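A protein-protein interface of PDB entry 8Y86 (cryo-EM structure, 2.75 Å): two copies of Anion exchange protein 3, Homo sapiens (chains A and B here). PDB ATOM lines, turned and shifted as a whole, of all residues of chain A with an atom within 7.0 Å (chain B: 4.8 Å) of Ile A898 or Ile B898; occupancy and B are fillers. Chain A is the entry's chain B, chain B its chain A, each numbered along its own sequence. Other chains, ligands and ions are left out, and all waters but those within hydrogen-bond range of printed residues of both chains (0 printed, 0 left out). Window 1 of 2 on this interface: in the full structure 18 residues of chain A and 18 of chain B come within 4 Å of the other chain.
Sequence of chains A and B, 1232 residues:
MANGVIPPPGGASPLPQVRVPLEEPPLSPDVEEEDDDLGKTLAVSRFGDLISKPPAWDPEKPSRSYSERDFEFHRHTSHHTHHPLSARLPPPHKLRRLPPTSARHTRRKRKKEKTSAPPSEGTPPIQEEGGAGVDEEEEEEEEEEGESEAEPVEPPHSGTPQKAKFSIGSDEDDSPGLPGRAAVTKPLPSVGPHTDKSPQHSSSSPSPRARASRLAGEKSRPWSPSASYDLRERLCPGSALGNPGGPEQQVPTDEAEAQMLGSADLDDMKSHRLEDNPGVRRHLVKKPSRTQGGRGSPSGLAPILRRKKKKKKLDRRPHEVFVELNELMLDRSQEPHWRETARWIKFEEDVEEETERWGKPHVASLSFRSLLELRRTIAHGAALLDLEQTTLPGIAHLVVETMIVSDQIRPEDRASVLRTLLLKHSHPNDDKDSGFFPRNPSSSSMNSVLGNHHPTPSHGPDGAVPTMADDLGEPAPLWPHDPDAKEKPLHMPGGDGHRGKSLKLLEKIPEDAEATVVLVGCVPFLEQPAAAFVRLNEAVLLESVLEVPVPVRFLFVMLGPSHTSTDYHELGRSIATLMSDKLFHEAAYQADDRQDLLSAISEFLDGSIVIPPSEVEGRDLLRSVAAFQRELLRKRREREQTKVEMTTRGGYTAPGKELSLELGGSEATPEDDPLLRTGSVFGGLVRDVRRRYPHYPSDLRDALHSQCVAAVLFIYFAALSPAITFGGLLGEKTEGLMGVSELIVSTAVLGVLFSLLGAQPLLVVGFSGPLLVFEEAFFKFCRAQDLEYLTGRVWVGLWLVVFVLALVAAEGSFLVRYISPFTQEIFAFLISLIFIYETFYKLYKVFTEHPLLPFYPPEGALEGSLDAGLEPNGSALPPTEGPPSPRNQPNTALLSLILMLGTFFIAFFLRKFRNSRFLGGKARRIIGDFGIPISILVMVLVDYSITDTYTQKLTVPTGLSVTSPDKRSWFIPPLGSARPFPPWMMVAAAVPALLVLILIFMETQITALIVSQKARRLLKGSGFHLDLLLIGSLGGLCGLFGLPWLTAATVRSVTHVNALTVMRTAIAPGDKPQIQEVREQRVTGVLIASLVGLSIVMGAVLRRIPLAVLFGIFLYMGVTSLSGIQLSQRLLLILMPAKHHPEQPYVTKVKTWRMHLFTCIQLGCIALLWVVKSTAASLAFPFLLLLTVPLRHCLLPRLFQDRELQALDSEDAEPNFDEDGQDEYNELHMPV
Among the printed residues, pairs that only touch across the chains: Leu A894 with Ile B898 (3.6 Å), Ile A898 with Leu B894 (3.6 Å), Leu A897 with Ile B898 (3.9 Å), Ile A898 with Leu B897 (3.9 Å) and Ile A898 with Ile B898 (3.9 Å).
Of the 18 printed residues of chain A, 3 touch a printed residue of chain B.
Printed residues of chain A that touch a printed residue of chain B: Leu A894, Leu A897 and Ile A898.
Hydrophobic or aromatic side chains of chain A that line the printed part of chain B: Leu A894, Leu A897 and Ile A898.
Printed residues of chain B that touch a printed residue of chain A: Leu B894, Leu B897 and Ile B898.
Hydrophobic or aromatic side chains of chain B that line the printed part of chain A: Leu B894, Leu B897 and Ile B898.
Among the printed residues, 5 pairs touch across the chains.
Among the printed residues, no Asp or Glu carboxylate lies within 4 Å of a Lys or Arg side-chain nitrogen of the other chain.
Of chain B, only Leu B894, Leu B897 and Ile B898 come within 4 Å of Ile A898.
Of chain A, only Leu A894, Leu A897 and Ile A898 come within 4 Å of Ile B898.
Of the printed residues of chain B, Leu A894 touches Ile B898 (3.6 Å).
Printed residues of chain A within 4 Å of Leu B897: Ile A898.
Of the printed residues of chain A, Leu B894 touches Ile A898.
Of the printed residues of chain B, Leu A897 touches Ile B898 (3.9 Å).
Gly B902 touches none of the printed residues of chain A.
The nearest printed residue of chain B that does not touch Ile A898 is Leu B895 (6.1 Å).
The nearest residue of chain A that does not touch Ile B898 is Leu A895 (6.1 Å).
Leu A894 touches Ile B898, and with the chains exchanged Ile A898 touches Leu B894.
Leu A897 touches Ile B898, and with the chains exchanged Ile A898 touches Leu B897.
Ile A898 touches its own counterpart, Ile B898.
Positions printed for both chains: 894, 895, 896, 897, 898, 899, 900, 901, 902 and 939.
Of the 5 pairs that touch across the chains among the printed residues, 5 have their exchanged pair printed and touching as well.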
ATOM      1  N   LEU A 843       9.619 -13.472 -24.963  1.00  0.00           N
ATOM      2  CA  LEU A 843       8.762 -12.782 -23.997  1.00  0.00           C
ATOM      3  C   LEU A 843       9.509 -11.640 -23.305  1.00  0.00           C
ATOM      4  O   LEU A 843       8.957 -10.546 -23.111  1.00  0.00           O
ATOM      5  CB  LEU A 843       8.215 -13.767 -22.966  1.00  0.00           C
ATOM      6  CG  LEU A 843       7.338 -13.132 -21.886  1.00  0.00           C
ATOM      7  CD1 LEU A 843       6.058 -12.582 -22.491  1.00  0.00           C
ATOM      8  CD2 LEU A 843       7.025 -14.131 -20.790  1.00  0.00           C
ATOM      9  N   PHE A 847       8.761  -7.561 -23.173  1.00  0.00           N
ATOM     10  CA  PHE A 847       8.752  -6.704 -21.987  1.00  0.00           C
ATOM     11  C   PHE A 847       9.653  -5.488 -22.165  1.00  0.00           C
ATOM     12  O   PHE A 847       9.303  -4.380 -21.743  1.00  0.00           O
ATOM     13  CB  PHE A 847       9.175  -7.482 -20.741  1.00  0.00           C
ATOM     14  CG  PHE A 847       8.079  -8.307 -20.134  1.00  0.00           C
ATOM     15  CD1 PHE A 847       6.887  -8.504 -20.800  1.00  0.00           C
ATOM     16  CD2 PHE A 847       8.227  -8.847 -18.872  1.00  0.00           C
ATOM     17  CE1 PHE A 847       5.878  -9.251 -20.233  1.00  0.00           C
ATOM     18  CE2 PHE A 847       7.217  -9.592 -18.302  1.00  0.00           C
ATOM     19  CZ  PHE A 847       6.042  -9.792 -18.983  1.00  0.00           C
ATOM     20  N   THR A 892       0.500  -3.514 -22.424  1.00  0.00           N
ATOM     21  CA  THR A 892       0.863  -4.450 -23.482  1.00  0.00           C
ATOM     22  C   THR A 892       1.649  -5.647 -22.955  1.00  0.00           C
ATOM     23  O   THR A 892       1.312  -6.797 -23.257  1.00  0.00           O
ATOM     24  CB  THR A 892       1.675  -3.731 -24.562  1.00  0.00           C
ATOM     25  OG1 THR A 892       0.890  -2.675 -25.125  1.00  0.00           O
ATOM     26  CG2 THR A 892       2.070  -4.695 -25.661  1.00  0.00           C
ATOM     27  N   ALA A 893       2.694  -5.390 -22.169  1.00  0.00           N
ATOM     28  CA  ALA A 893       3.553  -6.465 -21.684  1.00  0.00           C
ATOM     29  C   ALA A 893       2.791  -7.420 -20.772  1.00  0.00           C
ATOM     30  O   ALA A 893       2.883  -8.647 -20.913  1.00  0.00           O
ATOM     31  CB  ALA A 893       4.754  -5.867 -20.958  1.00  0.00           C
ATOM     32  N   LEU A 894       2.028  -6.871 -19.824  1.00  0.00           N
ATOM     33  CA  LEU A 894       1.293  -7.712 -18.888  1.00  0.00           C
ATOM     34  C   LEU A 894       0.205  -8.505 -19.601  1.00  0.00           C
ATOM     35  O   LEU A 894      -0.033  -9.674 -19.276  1.00  0.00           O
ATOM     36  CB  LEU A 894       0.701  -6.854 -17.771  1.00  0.00           C
ATOM     37  CG  LEU A 894       1.704  -6.170 -16.838  1.00  0.00           C
ATOM     38  CD1 LEU A 894       1.003  -5.156 -15.962  1.00  0.00           C
ATOM     39  CD2 LEU A 894       2.448  -7.183 -15.988  1.00  0.00           C
ATOM     40  N   LEU A 895      -0.461  -7.890 -20.580  1.00  0.00           N
ATOM     41  CA  LEU A 895      -1.474  -8.607 -21.346  1.00  0.00           C
ATOM     42  C   LEU A 895      -0.857  -9.738 -22.159  1.00  0.00           C
ATOM     43  O   LEU A 895      -1.439 -10.822 -22.267  1.00  0.00           O
ATOM     44  CB  LEU A 895      -2.228  -7.640 -22.257  1.00  0.00           C
ATOM     45  CG  LEU A 895      -3.461  -8.197 -22.965  1.00  0.00           C
ATOM     46  CD1 LEU A 895      -4.504  -8.636 -21.954  1.00  0.00           C
ATOM     47  CD2 LEU A 895      -4.035  -7.163 -23.914  1.00  0.00           C
ATOM     48  N   SER A 896       0.319  -9.503 -22.748  1.00  0.00           N
ATOM     49  CA  SER A 896       0.997 -10.564 -23.486  1.00  0.00           C
ATOM     50  C   SER A 896       1.377 -11.719 -22.568  1.00  0.00           C
ATOM     51  O   SER A 896       1.203 -12.894 -22.923  1.00  0.00           O
ATOM     52  CB  SER A 896       2.234 -10.005 -24.187  1.00  0.00           C
ATOM     53  OG  SER A 896       1.887  -8.931 -25.041  1.00  0.00           O
ATOM     54  N   LEU A 897       1.895 -11.403 -21.378  1.00  0.00           N
ATOM     55  CA  LEU A 897       2.220 -12.448 -20.411  1.00  0.00           C
ATOM     56  C   LEU A 897       0.978 -13.239 -20.016  1.00  0.00           C
ATOM     57  O   LEU A 897       1.016 -14.475 -19.925  1.00  0.00           O
ATOM     58  CB  LEU A 897       2.880 -11.825 -19.181  1.00  0.00           C
ATOM     59  CG  LEU A 897       3.084 -12.710 -17.954  1.00  0.00           C
ATOM     60  CD1 LEU A 897       4.086 -13.809 -18.249  1.00  0.00           C
ATOM     61  CD2 LEU A 897       3.541 -11.876 -16.772  1.00  0.00           C
ATOM     62  N   ILE A 898      -0.135 -12.540 -19.783  1.00  0.00           N
ATOM     63  CA  ILE A 898      -1.377 -13.205 -19.397  1.00  0.00           C
ATOM     64  C   ILE A 898      -1.864 -14.121 -20.511  1.00  0.00           C
ATOM     65  O   ILE A 898      -2.289 -15.253 -20.257  1.00  0.00           O
ATOM     66  CB  ILE A 898      -2.440 -12.159 -19.012  1.00  0.00           C
ATOM     67  CG1 ILE A 898      -2.161 -11.611 -17.614  1.00  0.00           C
ATOM     68  CG2 ILE A 898      -3.834 -12.755 -19.071  1.00  0.00           C
ATOM     69  CD1 ILE A 898      -3.047 -10.461 -17.228  1.00  0.00           C
ATOM     70  N   LEU A 899      -1.815 -13.651 -21.761  1.00  0.00           N
ATOM     71  CA  LEU A 899      -2.262 -14.474 -22.881  1.00  0.00           C
ATOM     72  C   LEU A 899      -1.405 -15.726 -23.024  1.00  0.00           C
ATOM     73  O   LEU A 899      -1.931 -16.830 -23.222  1.00  0.00           O
ATOM     74  CB  LEU A 899      -2.234 -13.664 -24.176  1.00  0.00           C
ATOM     75  CG  LEU A 899      -3.260 -12.542 -24.337  1.00  0.00           C
ATOM     76  CD1 LEU A 899      -2.994 -11.757 -25.610  1.00  0.00           C
ATOM     77  CD2 LEU A 899      -4.672 -13.093 -24.326  1.00  0.00           C
ATOM     78  N   MET A 900      -0.083 -15.574 -22.913  1.00  0.00           N
ATOM     79  CA  MET A 900       0.811 -16.725 -23.004  1.00  0.00           C
ATOM     80  C   MET A 900       0.500 -17.753 -21.921  1.00  0.00           C
ATOM     81  O   MET A 900       0.318 -18.948 -22.205  1.00  0.00           O
ATOM     82  CB  MET A 900       2.260 -16.252 -22.902  1.00  0.00           C
ATOM     83  CG  MET A 900       3.282 -17.356 -22.724  1.00  0.00           C
ATOM     84  SD  MET A 900       4.961 -16.753 -22.977  1.00  0.00           S
ATOM     85  CE  MET A 900       5.911 -18.241 -22.698  1.00  0.00           C
ATOM     86  N   LEU A 901       0.427 -17.300 -20.665  1.00  0.00           N
ATOM     87  CA  LEU A 901       0.191 -18.224 -19.562  1.00  0.00           C
ATOM     88  C   LEU A 901      -1.179 -18.880 -19.671  1.00  0.00           C
ATOM     89  O   LEU A 901      -1.324 -20.078 -19.399  1.00  0.00           O
ATOM     90  CB  LEU A 901       0.336 -17.497 -18.226  1.00  0.00           C
ATOM     91  CG  LEU A 901       1.767 -17.151 -17.812  1.00  0.00           C
ATOM     92  CD1 LEU A 901       1.797 -16.611 -16.392  1.00  0.00           C
ATOM     93  CD2 LEU A 901       2.673 -18.364 -17.947  1.00  0.00           C
ATOM     94  N   GLY A 902      -2.197 -18.115 -20.068  1.00  0.00           N
ATOM     95  CA  GLY A 902      -3.524 -18.685 -20.215  1.00  0.00           C
ATOM     96  C   GLY A 902      -3.588 -19.749 -21.291  1.00  0.00           C
ATOM     97  O   GLY A 902      -4.187 -20.808 -21.090  1.00  0.00           O
ATOM     98  N   THR A 903      -2.968 -19.489 -22.446  1.00  0.00           N
ATOM     99  CA  THR A 903      -2.946 -20.492 -23.506  1.00  0.00           C
ATOM    100  C   THR A 903      -2.256 -21.764 -23.034  1.00  0.00           C
ATOM    101  O   THR A 903      -2.779 -22.875 -23.212  1.00  0.00           O
ATOM    102  CB  THR A 903      -2.247 -19.937 -24.746  1.00  0.00           C
ATOM    103  OG1 THR A 903      -2.866 -18.706 -25.135  1.00  0.00           O
ATOM    104  CG2 THR A 903      -2.344 -20.921 -25.893  1.00  0.00           C
ATOM    105  N   PHE A 904      -1.086 -21.617 -22.402  1.00  0.00           N
ATOM    106  CA  PHE A 904      -0.356 -22.794 -21.940  1.00  0.00           C
ATOM    107  C   PHE A 904      -1.166 -23.590 -20.925  1.00  0.00           C
ATOM    108  O   PHE A 904      -1.248 -24.822 -21.012  1.00  0.00           O
ATOM    109  CB  PHE A 904       0.988 -22.379 -21.345  1.00  0.00           C
ATOM    110  CG  PHE A 904       1.743 -23.509 -20.707  1.00  0.00           C
ATOM    111  CD1 PHE A 904       2.350 -24.480 -21.484  1.00  0.00           C
ATOM    112  CD2 PHE A 904       1.848 -23.603 -19.331  1.00  0.00           C
ATOM    113  CE1 PHE A 904       3.045 -25.521 -20.900  1.00  0.00           C
ATOM    114  CE2 PHE A 904       2.542 -24.643 -18.744  1.00  0.00           C
ATOM    115  CZ  PHE A 904       3.141 -25.601 -19.531  1.00  0.00           C
ATOM    116  N   MET A 939      -8.401 -18.151 -26.493  1.00  0.00           N
ATOM    117  CA  MET A 939      -7.539 -17.017 -26.185  1.00  0.00           C
ATOM    118  C   MET A 939      -7.616 -15.940 -27.262  1.00  0.00           C
ATOM    119  O   MET A 939      -7.527 -14.748 -26.949  1.00  0.00           O
ATOM    120  CB  MET A 939      -6.101 -17.487 -25.990  1.00  0.00           C
ATOM    121  CG  MET A 939      -5.481 -16.974 -24.707  1.00  0.00           C
ATOM    122  SD  MET A 939      -6.348 -17.604 -23.257  1.00  0.00           S
ATOM    123  CE  MET A 939      -6.083 -16.269 -22.095  1.00  0.00           C
ATOM    124  N   VAL A 942     -10.721 -14.046 -26.459  1.00  0.00           N
ATOM    125  CA  VAL A 942     -10.490 -13.209 -25.283  1.00  0.00           C
ATOM    126  C   VAL A 942      -9.718 -11.951 -25.666  1.00  0.00           C
ATOM    127  O   VAL A 942     -10.055 -10.842 -25.233  1.00  0.00           O
ATOM    128  CB  VAL A 942      -9.760 -14.012 -24.190  1.00  0.00           C
ATOM    129  CG1 VAL A 942      -9.154 -13.081 -23.155  1.00  0.00           C
ATOM    130  CG2 VAL A 942     -10.711 -14.993 -23.530  1.00  0.00           C
ATOM    131  N   ALA A1108       1.341 -13.904 -28.605  1.00  0.00           N
ATOM    132  CA  ALA A1108       1.466 -14.491 -27.274  1.00  0.00           C
ATOM    133  C   ALA A1108       0.825 -15.873 -27.210  1.00  0.00           C
ATOM    134  O   ALA A1108       1.307 -16.759 -26.491  1.00  0.00           O
ATOM    135  CB  ALA A1108       0.849 -13.561 -26.233  1.00  0.00           C
ATOM    136  N   LEU B 894      -4.214  -5.369 -14.259  1.00  0.00           N
ATOM    137  CA  LEU B 894      -3.548  -6.570 -14.750  1.00  0.00           C
ATOM    138  C   LEU B 894      -2.514  -7.073 -13.752  1.00  0.00           C
ATOM    139  O   LEU B 894      -2.382  -8.285 -13.544  1.00  0.00           O
ATOM    140  CB  LEU B 894      -2.903  -6.289 -16.106  1.00  0.00           C
ATOM    141  CG  LEU B 894      -3.856  -5.997 -17.268  1.00  0.00           C
ATOM    142  CD1 LEU B 894      -3.084  -5.498 -18.469  1.00  0.00           C
ATOM    143  CD2 LEU B 894      -4.669  -7.223 -17.634  1.00  0.00           C
ATOM    144  N   LEU B 895      -1.778  -6.158 -13.118  1.00  0.00           N
ATOM    145  CA  LEU B 895      -0.807  -6.561 -12.106  1.00  0.00           C
ATOM    146  C   LEU B 895      -1.495  -7.186 -10.898  1.00  0.00           C
ATOM    147  O   LEU B 895      -0.994  -8.162 -10.330  1.00  0.00           O
ATOM    148  CB  LEU B 895       0.039  -5.363 -11.682  1.00  0.00           C
ATOM    149  CG  LEU B 895       1.241  -5.661 -10.789  1.00  0.00           C
ATOM    150  CD1 LEU B 895       2.229  -6.563 -11.506  1.00  0.00           C
ATOM    151  CD2 LEU B 895       1.909  -4.372 -10.357  1.00  0.00           C
ATOM    152  N   SER B 896      -2.637  -6.631 -10.485  1.00  0.00           N
ATOM    153  CA  SER B 896      -3.381  -7.216  -9.374  1.00  0.00           C
ATOM    154  C   SER B 896      -3.870  -8.619  -9.714  1.00  0.00           C
ATOM    155  O   SER B 896      -3.784  -9.536  -8.885  1.00  0.00           O
ATOM    156  CB  SER B 896      -4.556  -6.313  -9.000  1.00  0.00           C
ATOM    157  OG  SER B 896      -4.108  -5.008  -8.685  1.00  0.00           O
ATOM    158  N   LEU B 897      -4.384  -8.804 -10.931  1.00  0.00           N
ATOM    159  CA  LEU B 897      -4.809 -10.132 -11.365  1.00  0.00           C
ATOM    160  C   LEU B 897      -3.639 -11.110 -11.366  1.00  0.00           C
ATOM    161  O   LEU B 897      -3.773 -12.260 -10.923  1.00  0.00           O
ATOM    162  CB  LEU B 897      -5.443 -10.043 -12.752  1.00  0.00           C
ATOM    163  CG  LEU B 897      -5.743 -11.345 -13.494  1.00  0.00           C
ATOM    164  CD1 LEU B 897      -6.828 -12.127 -12.781  1.00  0.00           C
ATOM    165  CD2 LEU B 897      -6.148 -11.052 -14.925  1.00  0.00           C
ATOM    166  N   ILE B 898      -2.479 -10.664 -11.856  1.00  0.00           N
ATOM    167  CA  ILE B 898      -1.299 -11.524 -11.898  1.00  0.00           C
ATOM    168  C   ILE B 898      -0.869 -11.913 -10.489  1.00  0.00           C
ATOM    169  O   ILE B 898      -0.543 -13.076 -10.227  1.00  0.00           O
ATOM    170  CB  ILE B 898      -0.164 -10.827 -12.670  1.00  0.00           C
ATOM    171  CG1 ILE B 898      -0.418 -10.913 -14.174  1.00  0.00           C
ATOM    172  CG2 ILE B 898       1.181 -11.445 -12.333  1.00  0.00           C
ATOM    173  CD1 ILE B 898       0.551 -10.114 -14.996  1.00  0.00           C
ATOM    174  N   LEU B 899      -0.860 -10.952  -9.562  1.00  0.00           N
ATOM    175  CA  LEU B 899      -0.461 -11.248  -8.188  1.00  0.00           C
ATOM    176  C   LEU B 899      -1.412 -12.243  -7.537  1.00  0.00           C
ATOM    177  O   LEU B 899      -0.975 -13.193  -6.873  1.00  0.00           O
ATOM    178  CB  LEU B 899      -0.400  -9.961  -7.367  1.00  0.00           C
ATOM    179  CG  LEU B 899       0.714  -8.963  -7.685  1.00  0.00           C
ATOM    180  CD1 LEU B 899       0.538  -7.693  -6.872  1.00  0.00           C
ATOM    181  CD2 LEU B 899       2.079  -9.578  -7.439  1.00  0.00           C
ATOM    182  N   MET B 900      -2.720 -12.048  -7.725  1.00  0.00           N
ATOM    183  CA  MET B 900      -3.703 -12.969  -7.164  1.00  0.00           C
ATOM    184  C   MET B 900      -3.504 -14.384  -7.699  1.00  0.00           C
ATOM    185  O   MET B 900      -3.418 -15.352  -6.927  1.00  0.00           O
ATOM    186  CB  MET B 900      -5.110 -12.464  -7.480  1.00  0.00           C
ATOM    187  CG  MET B 900      -6.227 -13.444  -7.185  1.00  0.00           C
ATOM    188  SD  MET B 900      -7.842 -12.649  -7.267  1.00  0.00           S
ATOM    189  CE  MET B 900      -8.924 -14.024  -6.895  1.00  0.00           C
ATOM    190  N   LEU B 901      -3.418 -14.520  -9.025  1.00  0.00           N
ATOM    191  CA  LEU B 901      -3.278 -15.845  -9.622  1.00  0.00           C
ATOM    192  C   LEU B 901      -1.964 -16.498  -9.216  1.00  0.00           C
ATOM    193  O   LEU B 901      -1.921 -17.704  -8.945  1.00  0.00           O
ATOM    194  CB  LEU B 901      -3.389 -15.750 -11.141  1.00  0.00           C
ATOM    195  CG  LEU B 901      -4.793 -15.488 -11.687  1.00  0.00           C
ATOM    196  CD1 LEU B 901      -4.807 -15.590 -13.202  1.00  0.00           C
ATOM    197  CD2 LEU B 901      -5.797 -16.448 -11.070  1.00  0.00           C
ATOM    198  N   GLY B 902      -0.880 -15.722  -9.166  1.00  0.00           N
ATOM    199  CA  GLY B 902       0.397 -16.278  -8.761  1.00  0.00           C
ATOM    200  C   GLY B 902       0.390 -16.781  -7.332  1.00  0.00           C
ATOM    201  O   GLY B 902       0.892 -17.871  -7.049  1.00  0.00           O
ATOM    202  N   MET B 939       5.411 -13.524  -3.218  1.00  0.00           N
ATOM    203  CA  MET B 939       4.646 -12.562  -4.005  1.00  0.00           C
ATOM    204  C   MET B 939       4.847 -11.135  -3.508  1.00  0.00           C
ATOM    205  O   MET B 939       4.871 -10.199  -4.314  1.00  0.00           O
ATOM    206  CB  MET B 939       3.167 -12.934  -3.999  1.00  0.00           C
ATOM    207  CG  MET B 939       2.565 -12.976  -5.387  1.00  0.00           C
ATOM    208  SD  MET B 939       3.334 -14.250  -6.404  1.00  0.00           S
ATOM    209  CE  MET B 939       3.165 -13.535  -8.036  1.00  0.00           C
